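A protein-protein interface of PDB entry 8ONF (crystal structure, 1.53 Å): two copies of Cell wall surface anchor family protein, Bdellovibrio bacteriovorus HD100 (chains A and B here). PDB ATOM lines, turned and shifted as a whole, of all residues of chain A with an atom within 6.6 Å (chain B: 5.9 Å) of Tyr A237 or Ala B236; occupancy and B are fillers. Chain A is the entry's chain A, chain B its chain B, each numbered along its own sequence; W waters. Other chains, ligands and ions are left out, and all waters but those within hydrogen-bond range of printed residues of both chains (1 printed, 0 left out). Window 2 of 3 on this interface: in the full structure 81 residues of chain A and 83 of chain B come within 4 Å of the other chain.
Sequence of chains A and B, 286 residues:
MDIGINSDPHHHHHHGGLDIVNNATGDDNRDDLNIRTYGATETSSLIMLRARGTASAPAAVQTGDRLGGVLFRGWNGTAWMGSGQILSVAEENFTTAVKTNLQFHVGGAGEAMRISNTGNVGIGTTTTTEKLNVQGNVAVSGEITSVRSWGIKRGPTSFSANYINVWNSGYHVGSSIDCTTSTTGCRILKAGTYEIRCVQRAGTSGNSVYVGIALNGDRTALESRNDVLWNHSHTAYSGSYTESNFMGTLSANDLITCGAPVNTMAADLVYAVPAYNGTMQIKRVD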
ATOM      1  N   ARG A 201      -7.157  19.731  -5.810  1.00  0.00           N
ATOM      2  CA  ARG A 201      -7.464  18.310  -5.740  1.00  0.00           C
ATOM      3  C   ARG A 201      -6.999  17.676  -4.432  1.00  0.00           C
ATOM      4  O   ARG A 201      -5.878  17.903  -3.961  1.00  0.00           O
ATOM      5  CB  ARG A 201      -6.795  17.561  -6.893  1.00  0.00           C
ATOM      6  CG  ARG A 201      -7.468  17.769  -8.234  1.00  0.00           C
ATOM      7  CD  ARG A 201      -6.829  16.873  -9.288  1.00  0.00           C
ATOM      8  NE  ARG A 201      -7.509  17.048 -10.562  1.00  0.00           N
ATOM      9  CZ  ARG A 201      -7.356  16.243 -11.601  1.00  0.00           C
ATOM     10  NH1 ARG A 201      -6.556  15.181 -11.543  1.00  0.00           N
ATOM     11  NH2 ARG A 201      -8.052  16.481 -12.707  1.00  0.00           N
ATOM     12  N   ALA A 202      -7.857  16.830  -3.880  1.00  0.00           N
ATOM     13  CA  ALA A 202      -7.452  15.926  -2.810  1.00  0.00           C
ATOM     14  C   ALA A 202      -6.510  14.852  -3.347  1.00  0.00           C
ATOM     15  O   ALA A 202      -6.674  14.366  -4.472  1.00  0.00           O
ATOM     16  CB  ALA A 202      -8.682  15.266  -2.186  1.00  0.00           C
ATOM     17  N   GLY A 203      -5.532  14.471  -2.524  1.00  0.00           N
ATOM     18  CA  GLY A 203      -4.653  13.349  -2.810  1.00  0.00           C
ATOM     19  C   GLY A 203      -5.306  12.016  -2.521  1.00  0.00           C
ATOM     20  O   GLY A 203      -6.528  11.874  -2.609  1.00  0.00           O
ATOM     21  N   GLY A 206      -7.355   9.606   1.669  1.00  0.00           N
ATOM     22  CA  GLY A 206      -8.692   9.442   2.188  1.00  0.00           C
ATOM     23  C   GLY A 206      -9.060  10.354   3.337  1.00  0.00           C
ATOM     24  O   GLY A 206     -10.206  10.299   3.801  1.00  0.00           O
ATOM     25  N   ASN A 207      -8.140  11.201   3.805  1.00  0.00           N
ATOM     26  CA  ASN A 207      -8.435  12.125   4.891  1.00  0.00           C
ATOM     27  C   ASN A 207      -9.185  13.354   4.378  1.00  0.00           C
ATOM     28  O   ASN A 207      -9.102  13.728   3.209  1.00  0.00           O
ATOM     29  CB  ASN A 207      -7.145  12.597   5.560  1.00  0.00           C
ATOM     30  CG  ASN A 207      -6.386  11.470   6.229  1.00  0.00           C
ATOM     31  OD1 ASN A 207      -6.977  10.544   6.777  1.00  0.00           O
ATOM     32  ND2 ASN A 207      -5.058  11.568   6.220  1.00  0.00           N
ATOM     33  N   THR A 235     -13.298  17.977   1.212  1.00  0.00           N
ATOM     34  CA  THR A 235     -13.449  16.822   0.337  1.00  0.00           C
ATOM     35  C   THR A 235     -12.441  15.768   0.751  1.00  0.00           C
ATOM     36  O   THR A 235     -11.515  16.034   1.518  1.00  0.00           O
ATOM     37  CB  THR A 235     -13.285  17.188  -1.142  1.00  0.00           C
ATOM     38  OG1 THR A 235     -13.943  16.192  -1.937  1.00  0.00           O
ATOM     39  CG2 THR A 235     -11.807  17.283  -1.535  1.00  0.00           C
ATOM     40  N   ALA A 236     -12.641  14.551   0.250  1.00  0.00           N
ATOM     41  CA  ALA A 236     -11.676  13.481   0.492  1.00  0.00           C
ATOM     42  C   ALA A 236     -11.415  12.609  -0.727  1.00  0.00           C
ATOM     43  O   ALA A 236     -10.329  12.034  -0.814  1.00  0.00           O
ATOM     44  CB  ALA A 236     -12.121  12.583   1.655  1.00  0.00           C
ATOM     45  N   TYR A 237     -12.340  12.511  -1.674  1.00  0.00           N
ATOM     46  CA  TYR A 237     -12.163  11.608  -2.803  1.00  0.00           C
ATOM     47  C   TYR A 237     -10.974  12.046  -3.653  1.00  0.00           C
ATOM     48  O   TYR A 237     -10.836  13.225  -3.999  1.00  0.00           O
ATOM     49  CB  TYR A 237     -13.444  11.574  -3.645  1.00  0.00           C
ATOM     50  CG  TYR A 237     -13.413  10.573  -4.774  1.00  0.00           C
ATOM     51  CD1 TYR A 237     -13.634   9.228  -4.526  1.00  0.00           C
ATOM     52  CD2 TYR A 237     -13.145  10.970  -6.079  1.00  0.00           C
ATOM     53  CE1 TYR A 237     -13.606   8.310  -5.543  1.00  0.00           C
ATOM     54  CE2 TYR A 237     -13.110  10.061  -7.109  1.00  0.00           C
ATOM     55  CZ  TYR A 237     -13.343   8.725  -6.833  1.00  0.00           C
ATOM     56  OH  TYR A 237     -13.299   7.821  -7.873  1.00  0.00           O
ATOM     57  N   SER A 238     -10.127  11.091  -4.027  1.00  0.00           N
ATOM     58  CA  SER A 238      -8.908  11.433  -4.751  1.00  0.00           C
ATOM     59  C   SER A 238      -9.269  12.017  -6.112  1.00  0.00           C
ATOM     60  O   SER A 238     -10.015  11.406  -6.881  1.00  0.00           O
ATOM     61  CB  SER A 238      -8.035  10.189  -4.910  1.00  0.00           C
ATOM     62  OG  SER A 238      -7.016  10.397  -5.871  1.00  0.00           O
ATOM     63  N   GLY A 239      -8.758  13.222  -6.404  1.00  0.00           N
ATOM     64  CA  GLY A 239      -9.083  13.896  -7.643  1.00  0.00           C
ATOM     65  C   GLY A 239     -10.254  14.857  -7.562  1.00  0.00           C
ATOM     66  O   GLY A 239     -10.470  15.622  -8.509  1.00  0.00           O
ATOM     67  N   SER A 240     -11.015  14.836  -6.471  1.00  0.00           N
ATOM     68  CA  SER A 240     -12.093  15.794  -6.291  1.00  0.00           C
ATOM     69  C   SER A 240     -11.539  17.102  -5.740  1.00  0.00           C
ATOM     70  O   SER A 240     -10.434  17.156  -5.194  1.00  0.00           O
ATOM     71  CB  SER A 240     -13.163  15.240  -5.348  1.00  0.00           C
ATOM     72  OG  SER A 240     -12.668  15.155  -4.013  1.00  0.00           O
ATOM     73  N   TYR A 241     -12.349  18.135  -5.872  1.00  0.00           N
ATOM     74  CA  TYR A 241     -11.860  19.452  -5.448  1.00  0.00           C
ATOM     75  C   TYR A 241     -12.422  19.915  -4.116  1.00  0.00           C
ATOM     76  O   TYR A 241     -13.593  19.653  -3.842  1.00  0.00           O
ATOM     77  CB  TYR A 241     -12.377  20.529  -6.404  1.00  0.00           C
ATOM     78  CG  TYR A 241     -11.627  20.729  -7.694  1.00  0.00           C
ATOM     79  CD1 TYR A 241     -10.327  20.290  -7.846  1.00  0.00           C
ATOM     80  CD2 TYR A 241     -12.225  21.368  -8.767  1.00  0.00           C
ATOM     81  CE1 TYR A 241      -9.634  20.487  -9.026  1.00  0.00           C
ATOM     82  CE2 TYR A 241     -11.547  21.571  -9.955  1.00  0.00           C
ATOM     83  CZ  TYR A 241     -10.246  21.127 -10.087  1.00  0.00           C
ATOM     84  OH  TYR A 241      -9.541  21.315 -11.245  1.00  0.00           O
ATOM     85  N   ALA B 202     -22.132  12.004 -11.741  1.00  0.00           N
ATOM     86  CA  ALA B 202     -21.695  10.614 -11.727  1.00  0.00           C
ATOM     87  C   ALA B 202     -22.888   9.682 -11.593  1.00  0.00           C
ATOM     88  O   ALA B 202     -23.869   9.984 -10.901  1.00  0.00           O
ATOM     89  CB  ALA B 202     -20.730  10.361 -10.568  1.00  0.00           C
ATOM     90  N   GLY B 203     -22.782   8.520 -12.249  1.00  0.00           N
ATOM     91  CA  GLY B 203     -23.742   7.444 -12.093  1.00  0.00           C
ATOM     92  C   GLY B 203     -23.521   6.615 -10.845  1.00  0.00           C
ATOM     93  O   GLY B 203     -23.049   7.101  -9.815  1.00  0.00           O
ATOM     94  N   SER B 205     -21.844   3.514 -10.665  1.00  0.00           N
ATOM     95  CA  SER B 205     -20.780   2.523 -10.788  1.00  0.00           C
ATOM     96  C   SER B 205     -19.757   2.602  -9.664  1.00  0.00           C
ATOM     97  O   SER B 205     -19.100   1.600  -9.363  1.00  0.00           O
ATOM     98  CB  SER B 205     -20.086   2.694 -12.140  1.00  0.00           C
ATOM     99  OG  SER B 205     -19.070   3.688 -12.058  1.00  0.00           O
ATOM    100  N   GLY B 206     -19.590   3.767  -9.049  1.00  0.00           N
ATOM    101  CA  GLY B 206     -18.522   3.958  -8.099  1.00  0.00           C
ATOM    102  C   GLY B 206     -17.168   4.225  -8.715  1.00  0.00           C
ATOM    103  O   GLY B 206     -16.204   4.451  -7.971  1.00  0.00           O
ATOM    104  N   ASN B 207     -17.064   4.221 -10.043  1.00  0.00           N
ATOM    105  CA  ASN B 207     -15.816   4.541 -10.722  1.00  0.00           C
ATOM    106  C   ASN B 207     -15.553   6.045 -10.721  1.00  0.00           C
ATOM    107  O   ASN B 207     -16.469   6.867 -10.649  1.00  0.00           O
ATOM    108  CB  ASN B 207     -15.856   4.047 -12.163  1.00  0.00           C
ATOM    109  CG  ASN B 207     -15.829   2.537 -12.262  1.00  0.00           C
ATOM    110  OD1 ASN B 207     -15.182   1.867 -11.459  1.00  0.00           O
ATOM    111  ND2 ASN B 207     -16.535   1.997 -13.255  1.00  0.00           N
ATOM    112  N   SER B 208     -14.276   6.399 -10.839  1.00  0.00           N
ATOM    113  CA  SER B 208     -13.889   7.801 -10.998  1.00  0.00           C
ATOM    114  C   SER B 208     -14.283   8.293 -12.388  1.00  0.00           C
ATOM    115  O   SER B 208     -13.903   7.685 -13.397  1.00  0.00           O
ATOM    116  CB  SER B 208     -12.390   7.947 -10.793  1.00  0.00           C
ATOM    117  OG  SER B 208     -12.004   9.323 -10.898  1.00  0.00           O
ATOM    118  N   VAL B 209     -15.035   9.398 -12.449  1.00  0.00           N
ATOM    119  CA  VAL B 209     -15.474   9.961 -13.720  1.00  0.00           C
ATOM    120  C   VAL B 209     -15.112  11.439 -13.765  1.00  0.00           C
ATOM    121  O   VAL B 209     -14.941  12.104 -12.734  1.00  0.00           O
ATOM    122  CB  VAL B 209     -16.996   9.792 -13.968  1.00  0.00           C
ATOM    123  CG1 VAL B 209     -17.386   8.292 -14.012  1.00  0.00           C
ATOM    124  CG2 VAL B 209     -17.809  10.564 -12.920  1.00  0.00           C
ATOM    125  N   HIS B 234     -12.367  15.138 -10.677  1.00  0.00           N
ATOM    126  CA  HIS B 234     -12.950  13.804 -10.671  1.00  0.00           C
ATOM    127  C   HIS B 234     -13.996  13.691  -9.565  1.00  0.00           C
ATOM    128  O   HIS B 234     -13.899  14.359  -8.527  1.00  0.00           O
ATOM    129  CB  HIS B 234     -11.882  12.732 -10.417  1.00  0.00           C
ATOM    130  CG  HIS B 234     -10.858  12.605 -11.503  1.00  0.00           C
ATOM    131  ND1 HIS B 234     -10.851  11.551 -12.391  1.00  0.00           N
ATOM    132  CD2 HIS B 234      -9.784  13.370 -11.818  1.00  0.00           C
ATOM    133  CE1 HIS B 234      -9.829  11.679 -13.219  1.00  0.00           C
ATOM    134  NE2 HIS B 234      -9.166  12.775 -12.895  1.00  0.00           N
ATOM    135  N   THR B 235     -14.964  12.803  -9.774  1.00  0.00           N
ATOM    136  CA  THR B 235     -15.893  12.449  -8.711  1.00  0.00           C
ATOM    137  C   THR B 235     -16.353  11.008  -8.913  1.00  0.00           C
ATOM    138  O   THR B 235     -16.192  10.421  -9.988  1.00  0.00           O
ATOM    139  CB  THR B 235     -17.088  13.418  -8.660  1.00  0.00           C
ATOM    140  OG1 THR B 235     -17.666  13.396  -7.350  1.00  0.00           O
ATOM    141  CG2 THR B 235     -18.160  13.056  -9.681  1.00  0.00           C
ATOM    142  N   ALA B 236     -16.922  10.437  -7.862  1.00  0.00           N
ATOM    143  CA  ALA B 236     -17.505   9.110  -7.985  1.00  0.00           C
ATOM    144  C   ALA B 236     -18.873   8.976  -7.334  1.00  0.00           C
ATOM    145  O   ALA B 236     -19.667   8.155  -7.804  1.00  0.00           O
ATOM    146  CB  ALA B 236     -16.562   8.046  -7.403  1.00  0.00           C
ATOM    147  N   TYR B 237     -19.200   9.778  -6.318  1.00  0.00           N
ATOM    148  CA  TYR B 237     -20.434   9.581  -5.570  1.00  0.00           C
ATOM    149  C   TYR B 237     -21.640   9.817  -6.473  1.00  0.00           C
ATOM    150  O   TYR B 237     -21.678  10.779  -7.245  1.00  0.00           O
ATOM    151  CB  TYR B 237     -20.484  10.533  -4.375  1.00  0.00           C
ATOM    152  CG  TYR B 237     -21.681  10.296  -3.482  1.00  0.00           C
ATOM    153  CD1 TYR B 237     -21.719   9.204  -2.635  1.00  0.00           C
ATOM    154  CD2 TYR B 237     -22.795  11.140  -3.526  1.00  0.00           C
ATOM    155  CE1 TYR B 237     -22.817   8.967  -1.822  1.00  0.00           C
ATOM    156  CE2 TYR B 237     -23.902  10.902  -2.721  1.00  0.00           C
ATOM    157  CZ  TYR B 237     -23.903   9.815  -1.876  1.00  0.00           C
ATOM    158  OH  TYR B 237     -24.996   9.578  -1.073  1.00  0.00           O
ATOM    159  N   SER B 238     -22.650   8.958  -6.349  1.00  0.00           N
ATOM    160  CA  SER B 238     -23.782   9.034  -7.260  1.00  0.00           C
ATOM    161  C   SER B 238     -24.507  10.373  -7.092  1.00  0.00           C
ATOM    162  O   SER B 238     -24.869  10.775  -5.982  1.00  0.00           O
ATOM    163  CB  SER B 238     -24.728   7.844  -7.024  1.00  0.00           C
ATOM    164  OG  SER B 238     -26.012   8.063  -7.587  1.00  0.00           O
ATOM    165  N   GLY B 239     -24.704  11.074  -8.206  1.00  0.00           N
ATOM    166  CA  GLY B 239     -25.370  12.358  -8.192  1.00  0.00           C
ATOM    167  C   GLY B 239     -24.477  13.543  -7.894  1.00  0.00           C
ATOM    168  O   GLY B 239     -24.935  14.683  -7.996  1.00  0.00           O
ATOM    169  N   SER B 240     -23.221  13.313  -7.530  1.00  0.00           N
ATOM    170  CA  SER B 240     -22.279  14.405  -7.363  1.00  0.00           C
ATOM    171  C   SER B 240     -21.788  14.876  -8.725  1.00  0.00           C
ATOM    172  O   SER B 240     -21.919  14.177  -9.733  1.00  0.00           O
ATOM    173  CB  SER B 240     -21.113  13.959  -6.480  1.00  0.00           C
ATOM    174  OG  SER B 240     -20.318  12.981  -7.141  1.00  0.00           O
HETATM  175  O   HOH W   1     -13.555   5.241  -7.350  1.00  0.00           O
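The backbone NH of Gly A239 lies within hydrogen-bond range of the backbone carbonyl oxygen of Ala A202 (3.1 Å).
The backbone carbonyl oxygen (O) of Ser A240 lies within hydrogen-bond range of the backbone NH (N) of Ala A202, 2.9 Å away.
O of Tyr A237 lies within hydrogen-bond range of OG of Ser A240 (2.7 Å).
OG of Ser B208 sits at hydrogen-bond distance from ND1 of His B234 (2.9 Å).
N of Val B209 lies within hydrogen-bond range of O of Thr B235 (2.9 Å).
The side-chain hydroxyl of Ser B240 is in hydrogen-bond range of the side-chain hydroxyl of Thr B235 (2.7 Å).
Gly A203 touches none of the printed residues of chain B.
Ala A236 touches none of the printed residues of chain B.
Of chain B, only Ser B208 (3.1 Å), Thr B235 (3.8 Å) and Ala B236 (3.3 Å) come within 4 Å of Tyr A237.
Of the printed residues of chain B, Gly A239 touches His B234 (2.9 Å).
Of the printed residues of chain B, Ser A240 touches His B234 (3.2 Å).
Printed residues of chain A within 4 Å of Thr B235: Tyr A237 (3.8 Å).
Ala B236 touches just one residue of chain A: Tyr A237.
Among the printed residues, merely in contact across the chains: Ser A240 with His B234, Tyr A237 with Ala B236, Arg A201 with His B234 and Tyr A237 with Thr B235.
Hydrophobic or aromatic side chains of chain B within 4 Å of the printed part of chain A: His B234 and Ala B236.
Along chain B the printed residues that touch a printed residue of chain A span positions 208 to 236.
Among the printed residues, 6 pairs touch across the chains.
Among the printed residues, no Asp or Glu carboxylate lies within 4 Å of a Lys or Arg side-chain nitrogen of the other chain.
Water W1 lies within hydrogen-bond range of the side-chain hydroxyl of Tyr A237 and the backbone carbonyl oxygen of Gly B206.
The side-chain hydroxyl of Tyr A237 lies close to the backbone NH of Ser B208, 3.4 Å away.
The backbone NH (N) of His B234 sits at hydrogen-bond distance from the backbone carbonyl oxygen (O) of Gly A239.
Tyr A237 touches Thr B235, but with the chains exchanged Thr A235 does not touch Tyr B237 (9.0 Å).
Tyr A237 touches Ala B236, but with the chains exchanged Ala A236 does not touch Tyr B237 (10.0 Å).
Positions printed for both chains: 202, 203, 206, 207, 235, 236, 237, 238, 239 and 240.
Of the 6 pairs that touch across the chains among the printed residues, none has its exchanged pair printed and touching as well.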
